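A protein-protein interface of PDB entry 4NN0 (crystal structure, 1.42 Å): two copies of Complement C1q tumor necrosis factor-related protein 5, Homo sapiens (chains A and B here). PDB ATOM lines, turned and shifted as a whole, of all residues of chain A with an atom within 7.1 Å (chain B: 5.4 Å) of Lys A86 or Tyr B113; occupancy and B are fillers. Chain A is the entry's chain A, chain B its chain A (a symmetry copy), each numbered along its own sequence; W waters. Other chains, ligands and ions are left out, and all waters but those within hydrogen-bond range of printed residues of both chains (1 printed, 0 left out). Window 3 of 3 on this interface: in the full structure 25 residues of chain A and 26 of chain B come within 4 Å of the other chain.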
ATOM      1  N   THR A  57       5.748 -12.696 -27.575  1.00  0.00           N
ATOM      2  CA  THR A  57       5.303 -11.410 -27.147  1.00  0.00           C
ATOM      3  C   THR A  57       4.090 -11.003 -27.998  1.00  0.00           C
ATOM      4  O   THR A  57       4.095 -11.251 -29.213  1.00  0.00           O
ATOM      5  CB  THR A  57       6.472 -10.391 -27.202  1.00  0.00           C
ATOM      6  OG1 THR A  57       7.547 -10.829 -26.370  1.00  0.00           O
ATOM      7  CG2 THR A  57       6.025  -9.058 -26.751  1.00  0.00           C
ATOM      8  N   VAL A  58       3.073 -10.413 -27.373  1.00  0.00           N
ATOM      9  CA  VAL A  58       1.790 -10.086 -28.009  1.00  0.00           C
ATOM     10  C   VAL A  58       1.608  -8.585 -27.945  1.00  0.00           C
ATOM     11  O   VAL A  58       1.621  -7.996 -26.866  1.00  0.00           O
ATOM     12  CB  VAL A  58       0.628 -10.773 -27.254  1.00  0.00           C
ATOM     13  CG1 VAL A  58      -0.734 -10.435 -27.876  1.00  0.00           C
ATOM     14  CG2 VAL A  58       0.872 -12.280 -27.234  1.00  0.00           C
ATOM     15  N   TYR A  59       1.374  -7.916 -29.072  1.00  0.00           N
ATOM     16  CA  TYR A  59       1.202  -6.484 -29.058  1.00  0.00           C
ATOM     17  C   TYR A  59       0.428  -6.014 -30.300  1.00  0.00           C
ATOM     18  O   TYR A  59       0.593  -6.578 -31.375  1.00  0.00           O
ATOM     19  CB  TYR A  59       2.571  -5.794 -29.020  1.00  0.00           C
ATOM     20  CG  TYR A  59       2.582  -4.323 -28.719  1.00  0.00           C
ATOM     21  CD1 TYR A  59       1.912  -3.789 -27.642  1.00  0.00           C
ATOM     22  CD2 TYR A  59       3.327  -3.461 -29.482  1.00  0.00           C
ATOM     23  CE1 TYR A  59       1.950  -2.436 -27.342  1.00  0.00           C
ATOM     24  CE2 TYR A  59       3.395  -2.116 -29.191  1.00  0.00           C
ATOM     25  CZ  TYR A  59       2.713  -1.594 -28.114  1.00  0.00           C
ATOM     26  OH  TYR A  59       2.753  -0.245 -27.792  1.00  0.00           O
ATOM     27  N   ARG A  60      -0.413  -5.014 -30.096  1.00  0.00           N
ATOM     28  CA  ARG A  60      -1.212  -4.320 -31.092  1.00  0.00           C
ATOM     29  C   ARG A  60      -2.455  -5.042 -31.613  1.00  0.00           C
ATOM     30  O   ARG A  60      -3.286  -4.427 -32.252  1.00  0.00           O
ATOM     31  CB  ARG A  60      -0.419  -3.855 -32.343  1.00  0.00           C
ATOM     32  CG  ARG A  60       0.833  -3.014 -31.995  1.00  0.00           C
ATOM     33  CD  ARG A  60       1.341  -2.192 -33.149  1.00  0.00           C
ATOM     34  NE  ARG A  60       2.619  -1.550 -32.873  1.00  0.00           N
ATOM     35  CZ  ARG A  60       2.756  -0.455 -32.131  1.00  0.00           C
ATOM     36  NH1 ARG A  60       1.685   0.124 -31.602  1.00  0.00           N
ATOM     37  NH2 ARG A  60       3.978   0.038 -31.953  1.00  0.00           N
ATOM     38  N   PHE A  81      -5.523  -9.277 -26.428  1.00  0.00           N
ATOM     39  CA  PHE A  81      -4.771  -8.045 -26.278  1.00  0.00           C
ATOM     40  C   PHE A  81      -5.774  -6.893 -26.087  1.00  0.00           C
ATOM     41  O   PHE A  81      -6.323  -6.337 -27.045  1.00  0.00           O
ATOM     42  CB  PHE A  81      -3.872  -7.735 -27.482  1.00  0.00           C
ATOM     43  CG  PHE A  81      -2.989  -6.557 -27.213  1.00  0.00           C
ATOM     44  CD1 PHE A  81      -1.906  -6.682 -26.351  1.00  0.00           C
ATOM     45  CD2 PHE A  81      -3.269  -5.306 -27.721  1.00  0.00           C
ATOM     46  CE1 PHE A  81      -1.142  -5.573 -26.030  1.00  0.00           C
ATOM     47  CE2 PHE A  81      -2.492  -4.200 -27.396  1.00  0.00           C
ATOM     48  CZ  PHE A  81      -1.449  -4.360 -26.521  1.00  0.00           C
ATOM     49  N   GLY A  83      -6.156  -3.678 -25.613  1.00  0.00           N
ATOM     50  CA  GLY A  83      -5.999  -2.255 -25.748  1.00  0.00           C
ATOM     51  C   GLY A  83      -4.991  -1.674 -24.772  1.00  0.00           C
ATOM     52  O   GLY A  83      -5.133  -0.514 -24.346  1.00  0.00           O
ATOM     53  N   TRP A  84      -3.968  -2.452 -24.429  1.00  0.00           N
ATOM     54  CA  TRP A  84      -2.930  -2.033 -23.470  1.00  0.00           C
ATOM     55  C   TRP A  84      -1.788  -1.266 -24.151  1.00  0.00           C
ATOM     56  O   TRP A  84      -1.523  -1.423 -25.354  1.00  0.00           O
ATOM     57  CB  TRP A  84      -2.407  -3.255 -22.718  1.00  0.00           C
ATOM     58  CG  TRP A  84      -3.488  -3.986 -21.990  1.00  0.00           C
ATOM     59  CD1 TRP A  84      -4.410  -3.452 -21.161  1.00  0.00           C
ATOM     60  CD2 TRP A  84      -3.777  -5.385 -22.069  1.00  0.00           C
ATOM     61  NE1 TRP A  84      -5.278  -4.443 -20.703  1.00  0.00           N
ATOM     62  CE2 TRP A  84      -4.890  -5.628 -21.246  1.00  0.00           C
ATOM     63  CE3 TRP A  84      -3.174  -6.468 -22.707  1.00  0.00           C
ATOM     64  CZ2 TRP A  84      -5.450  -6.903 -21.113  1.00  0.00           C
ATOM     65  CZ3 TRP A  84      -3.726  -7.734 -22.574  1.00  0.00           C
ATOM     66  CH2 TRP A  84      -4.846  -7.933 -21.767  1.00  0.00           C
ATOM     67  N   PRO A  85      -1.038  -0.444 -23.382  1.00  0.00           N
ATOM     68  CA  PRO A  85      -0.009   0.390 -24.007  1.00  0.00           C
ATOM     69  C   PRO A  85       1.303  -0.360 -24.264  1.00  0.00           C
ATOM     70  O   PRO A  85       2.175   0.188 -24.946  1.00  0.00           O
ATOM     71  CB  PRO A  85       0.172   1.528 -22.999  1.00  0.00           C
ATOM     72  CG  PRO A  85      -0.208   0.912 -21.665  1.00  0.00           C
ATOM     73  CD  PRO A  85      -1.415   0.082 -22.052  1.00  0.00           C
ATOM     74  N   LYS A  86       1.456  -1.576 -23.729  1.00  0.00           N
ATOM     75  CA  LYS A  86       2.680  -2.334 -23.814  1.00  0.00           C
ATOM     76  C   LYS A  86       2.337  -3.800 -23.986  1.00  0.00           C
ATOM     77  O   LYS A  86       1.161  -4.161 -23.848  1.00  0.00           O
ATOM     78  CB  LYS A  86       3.507  -2.179 -22.549  1.00  0.00           C
ATOM     79  CG  LYS A  86       3.922  -0.746 -22.355  1.00  0.00           C
ATOM     80  CD  LYS A  86       4.578  -0.597 -21.000  1.00  0.00           C
ATOM     81  CE  LYS A  86       4.776   0.833 -20.740  1.00  0.00           C
ATOM     82  NZ  LYS A  86       5.451   1.003 -19.470  1.00  0.00           N
ATOM     83  N   PRO A  87       3.311  -4.650 -24.338  1.00  0.00           N
ATOM     84  CA  PRO A  87       2.952  -6.011 -24.739  1.00  0.00           C
ATOM     85  C   PRO A  87       2.487  -6.928 -23.630  1.00  0.00           C
ATOM     86  O   PRO A  87       2.836  -6.774 -22.462  1.00  0.00           O
ATOM     87  CB  PRO A  87       4.235  -6.555 -25.354  1.00  0.00           C
ATOM     88  CG  PRO A  87       4.991  -5.329 -25.809  1.00  0.00           C
ATOM     89  CD  PRO A  87       4.688  -4.303 -24.753  1.00  0.00           C
ATOM     90  N   ALA A  88       1.692  -7.921 -24.022  1.00  0.00           N
ATOM     91  CA  ALA A  88       1.395  -9.110 -23.257  1.00  0.00           C
ATOM     92  C   ALA A  88       2.222 -10.294 -23.776  1.00  0.00           C
ATOM     93  O   ALA A  88       3.188 -10.114 -24.520  1.00  0.00           O
ATOM     94  CB  ALA A  88      -0.101  -9.386 -23.271  1.00  0.00           C
ATOM     95  N   LYS A 121      13.739  -5.030 -26.466  1.00  0.00           N
ATOM     96  CA  LYS A 121      13.766  -5.833 -25.221  1.00  0.00           C
ATOM     97  C   LYS A 121      12.639  -6.868 -25.135  1.00  0.00           C
ATOM     98  O   LYS A 121      12.301  -7.308 -24.037  1.00  0.00           O
ATOM     99  CB  LYS A 121      13.773  -4.937 -23.978  1.00  0.00           C
ATOM    100  CG  LYS A 121      15.024  -4.068 -23.819  1.00  0.00           C
ATOM    101  CD  LYS A 121      16.310  -4.825 -23.776  1.00  0.00           C
ATOM    102  CE  LYS A 121      16.455  -5.842 -22.687  1.00  0.00           C
ATOM    103  NZ  LYS A 121      17.901  -6.353 -22.586  1.00  0.00           N
ATOM    104  N   ALA B  61       4.290  -4.837 -10.654  1.00  0.00           N
ATOM    105  CA  ALA B  61       5.002  -4.094 -11.676  1.00  0.00           C
ATOM    106  C   ALA B  61       5.039  -5.015 -12.886  1.00  0.00           C
ATOM    107  O   ALA B  61       4.941  -6.229 -12.721  1.00  0.00           O
ATOM    108  CB  ALA B  61       6.439  -3.719 -11.263  1.00  0.00           C
ATOM    109  N   SER B  62       5.216  -4.450 -14.084  1.00  0.00           N
ATOM    110  CA  SER B  62       5.505  -5.279 -15.207  1.00  0.00           C
ATOM    111  C   SER B  62       6.808  -6.050 -15.026  1.00  0.00           C
ATOM    112  O   SER B  62       7.652  -5.625 -14.206  1.00  0.00           O
ATOM    113  CB  SER B  62       5.586  -4.472 -16.481  1.00  0.00           C
ATOM    114  OG  SER B  62       4.355  -3.823 -16.774  1.00  0.00           O
ATOM    115  N   LEU B  63       6.996  -7.153 -15.756  1.00  0.00           N
ATOM    116  CA  LEU B  63       8.190  -7.943 -15.688  1.00  0.00           C
ATOM    117  C   LEU B  63       8.841  -8.007 -17.050  1.00  0.00           C
ATOM    118  O   LEU B  63       8.196  -8.370 -18.026  1.00  0.00           O
ATOM    119  CB  LEU B  63       7.933  -9.377 -15.176  1.00  0.00           C
ATOM    120  CG  LEU B  63       9.112 -10.291 -15.133  1.00  0.00           C
ATOM    121  CD1 LEU B  63      10.253  -9.784 -14.244  1.00  0.00           C
ATOM    122  CD2 LEU B  63       8.646 -11.689 -14.670  1.00  0.00           C
ATOM    123  N   GLN B  64      10.123  -7.644 -17.103  1.00  0.00           N
ATOM    124  CA  GLN B  64      10.972  -7.839 -18.244  1.00  0.00           C
ATOM    125  C   GLN B  64      12.142  -8.687 -17.791  1.00  0.00           C
ATOM    126  O   GLN B  64      12.791  -8.355 -16.786  1.00  0.00           O
ATOM    127  CB  GLN B  64      11.438  -6.502 -18.836  1.00  0.00           C
ATOM    128  CG  GLN B  64      12.025  -6.623 -20.264  1.00  0.00           C
ATOM    129  CD  GLN B  64      13.429  -7.227 -20.291  1.00  0.00           C
ATOM    130  OE1 GLN B  64      14.228  -7.093 -19.317  1.00  0.00           O
ATOM    131  NE2 GLN B  64      13.751  -7.909 -21.320  1.00  0.00           N
ATOM    132  N   PHE B  78       8.647 -10.091 -21.865  1.00  0.00           N
ATOM    133  CA  PHE B  78       7.948  -9.025 -21.192  1.00  0.00           C
ATOM    134  C   PHE B  78       6.486  -9.315 -21.009  1.00  0.00           C
ATOM    135  O   PHE B  78       5.821  -9.862 -21.917  1.00  0.00           O
ATOM    136  CB  PHE B  78       8.098  -7.712 -21.982  1.00  0.00           C
ATOM    137  CG  PHE B  78       7.352  -6.529 -21.356  1.00  0.00           C
ATOM    138  CD1 PHE B  78       7.972  -5.758 -20.354  1.00  0.00           C
ATOM    139  CD2 PHE B  78       6.057  -6.186 -21.702  1.00  0.00           C
ATOM    140  CE1 PHE B  78       7.298  -4.711 -19.755  1.00  0.00           C
ATOM    141  CE2 PHE B  78       5.395  -5.156 -21.118  1.00  0.00           C
ATOM    142  CZ  PHE B  78       6.018  -4.390 -20.149  1.00  0.00           C
ATOM    143  N   PHE B  80       3.140  -6.945 -19.493  1.00  0.00           N
ATOM    144  CA  PHE B  80       2.498  -5.774 -18.937  1.00  0.00           C
ATOM    145  C   PHE B  80       1.747  -6.119 -17.677  1.00  0.00           C
ATOM    146  O   PHE B  80       0.946  -7.087 -17.686  1.00  0.00           O
ATOM    147  CB  PHE B  80       1.519  -5.240 -19.990  1.00  0.00           C
ATOM    148  CG  PHE B  80       0.753  -4.015 -19.609  1.00  0.00           C
ATOM    149  CD1 PHE B  80       1.384  -2.802 -19.395  1.00  0.00           C
ATOM    150  CD2 PHE B  80      -0.620  -4.059 -19.515  1.00  0.00           C
ATOM    151  CE1 PHE B  80       0.647  -1.693 -19.089  1.00  0.00           C
ATOM    152  CE2 PHE B  80      -1.361  -2.925 -19.191  1.00  0.00           C
ATOM    153  CZ  PHE B  80      -0.712  -1.736 -18.989  1.00  0.00           C
ATOM    154  N   VAL B 108      16.648  -9.162 -14.855  1.00  0.00           N
ATOM    155  CA  VAL B 108      15.813  -8.069 -15.326  1.00  0.00           C
ATOM    156  C   VAL B 108      16.668  -7.184 -16.242  1.00  0.00           C
ATOM    157  O   VAL B 108      17.717  -6.722 -15.816  1.00  0.00           O
ATOM    158  CB  VAL B 108      15.201  -7.239 -14.170  1.00  0.00           C
ATOM    159  CG1 VAL B 108      14.512  -6.022 -14.662  1.00  0.00           C
ATOM    160  CG2 VAL B 108      14.281  -8.121 -13.366  1.00  0.00           C
ATOM    161  N   VAL B 110      15.486  -4.266 -18.045  1.00  0.00           N
ATOM    162  CA  VAL B 110      15.008  -2.889 -18.004  1.00  0.00           C
ATOM    163  C   VAL B 110      14.635  -2.676 -16.553  1.00  0.00           C
ATOM    164  O   VAL B 110      13.715  -3.323 -16.054  1.00  0.00           O
ATOM    165  CB  VAL B 110      13.829  -2.616 -18.941  1.00  0.00           C
ATOM    166  CG1 VAL B 110      13.373  -1.161 -18.803  1.00  0.00           C
ATOM    167  CG2 VAL B 110      14.169  -2.945 -20.387  1.00  0.00           C
ATOM    168  N   GLY B 111      15.377  -1.804 -15.859  1.00  0.00           N
ATOM    169  CA  GLY B 111      15.522  -1.936 -14.434  1.00  0.00           C
ATOM    170  C   GLY B 111      14.369  -1.629 -13.511  1.00  0.00           C
ATOM    171  O   GLY B 111      14.499  -1.847 -12.307  1.00  0.00           O
ATOM    172  N   ASP B 112      13.245  -1.140 -14.024  1.00  0.00           N
ATOM    173  CA  ASP B 112      12.041  -0.959 -13.242  1.00  0.00           C
ATOM    174  C   ASP B 112      10.979  -2.031 -13.519  1.00  0.00           C
ATOM    175  O   ASP B 112       9.936  -2.040 -12.862  1.00  0.00           O
ATOM    176  CB  ASP B 112      11.415   0.425 -13.432  1.00  0.00           C
ATOM    177  CG  ASP B 112      11.040   0.743 -14.853  1.00  0.00           C
ATOM    178  OD1 ASP B 112      11.598   0.142 -15.783  1.00  0.00           O
ATOM    179  OD2 ASP B 112      10.177   1.630 -15.037  1.00  0.00           O
ATOM    180  N   TYR B 113      11.239  -2.941 -14.441  1.00  0.00           N
ATOM    181  CA  TYR B 113      10.251  -3.973 -14.789  1.00  0.00           C
ATOM    182  C   TYR B 113      10.585  -5.212 -13.977  1.00  0.00           C
ATOM    183  O   TYR B 113      11.000  -6.263 -14.497  1.00  0.00           O
ATOM    184  CB  TYR B 113      10.294  -4.219 -16.286  1.00  0.00           C
ATOM    185  CG  TYR B 113       9.703  -3.123 -17.141  1.00  0.00           C
ATOM    186  CD1 TYR B 113       8.658  -2.323 -16.701  1.00  0.00           C
ATOM    187  CD2 TYR B 113      10.171  -2.923 -18.435  1.00  0.00           C
ATOM    188  CE1 TYR B 113       8.048  -1.413 -17.553  1.00  0.00           C
ATOM    189  CE2 TYR B 113       9.589  -2.009 -19.297  1.00  0.00           C
ATOM    190  CZ  TYR B 113       8.534  -1.251 -18.854  1.00  0.00           C
ATOM    191  OH  TYR B 113       7.907  -0.348 -19.678  1.00  0.00           O
ATOM    192  N   ILE B 114      10.388  -5.063 -12.672  1.00  0.00           N
ATOM    193  CA  ILE B 114      10.900  -5.972 -11.684  1.00  0.00           C
ATOM    194  C   ILE B 114       9.822  -6.862 -11.035  1.00  0.00           C
ATOM    195  O   ILE B 114      10.043  -7.437  -9.976  1.00  0.00           O
ATOM    196  CB  ILE B 114      11.542  -5.161 -10.518  1.00  0.00           C
ATOM    197  CG1 ILE B 114      10.495  -4.261  -9.809  1.00  0.00           C
ATOM    198  CG2 ILE B 114      12.745  -4.381 -11.057  1.00  0.00           C
ATOM    199  CD1 ILE B 114      11.028  -3.447  -8.641  1.00  0.00           C
ATOM    200  N   GLY B 115       8.679  -7.011 -11.688  1.00  0.00           N
ATOM    201  CA  GLY B 115       7.522  -7.685 -11.117  1.00  0.00           C
ATOM    202  C   GLY B 115       7.487  -9.181 -11.002  1.00  0.00           C
ATOM    203  O   GLY B 115       6.389  -9.757 -11.000  1.00  0.00           O
HETATM  204  O   HOH W   1       7.032 -11.689 -23.745  1.00  0.00           O
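N of Phe B80 sits at hydrogen-bond distance from O of Pro A87 (3.0 Å). NE2 of Gln B64 is in hydrogen-bond range of O of Lys A121 (3.1 Å). The side-chain amino group (NZ) of Lys A86 lies within hydrogen-bond range of the side-chain hydroxyl (OH) of Tyr B113, at 2.8 Å.
O of Pro A85 lies within hydrogen-bond range of OH of Tyr A59 (2.9 Å). The side-chain amide oxygen of Gln B64 sits at hydrogen-bond distance from the backbone NH of Val B110 (3.3 Å). The backbone NH (N) of Ala A88 sits at hydrogen-bond distance from the backbone carbonyl oxygen (O) of Val A58, 2.8 Å away. The backbone NH of Gln B64 sits at hydrogen-bond distance from the backbone carbonyl oxygen of Tyr B113.
Among the printed residues, pairs that only touch across the chains: Trp A84 with Phe B80, Pro A85 with Phe B80, Lys A86 with Phe B78, Lys A86 with Phe B80, Pro A87 with Phe B78, Ala A88 with Phe B78 and Lys A121 with Val B110.
Thr A57 touches none of the printed residues of chain B. Of the printed residues of chain B, Pro A85 touches Phe B80 (3.6 Å). Printed residues of chain B within 4 Å of Pro A87: Phe B78 and Phe B80. Printed residues of chain B within 4 Å of Ala A88: Phe B78 (3.7 Å). Leu B63 touches none of the printed residues of chain A. The nearest residue of chain B that does not touch Lys A86 is Ser B62 (5.3 Å). The nearest printed residue of chain B that does not touch Trp A84 is Phe B78 (8.2 Å).
Hydrophobic or aromatic side chains of chain A that line the printed part of chain B: Trp A84, Pro A85 and Pro A87. Among the printed residues, no Asp or Glu carboxylate lies within 4 Å of a Lys or Arg side-chain nitrogen of the other chain.
No position is printed for both chains. Of the 10 pairs that touch across the chains among the printed residues, none has its exchanged pair printed and touching as well.
Water W1 bridges the side-chain hydroxyl (OG1) of Thr A57 (2.8 Å) and the backbone carbonyl oxygen (O) of Phe B78 (2.9 Å).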
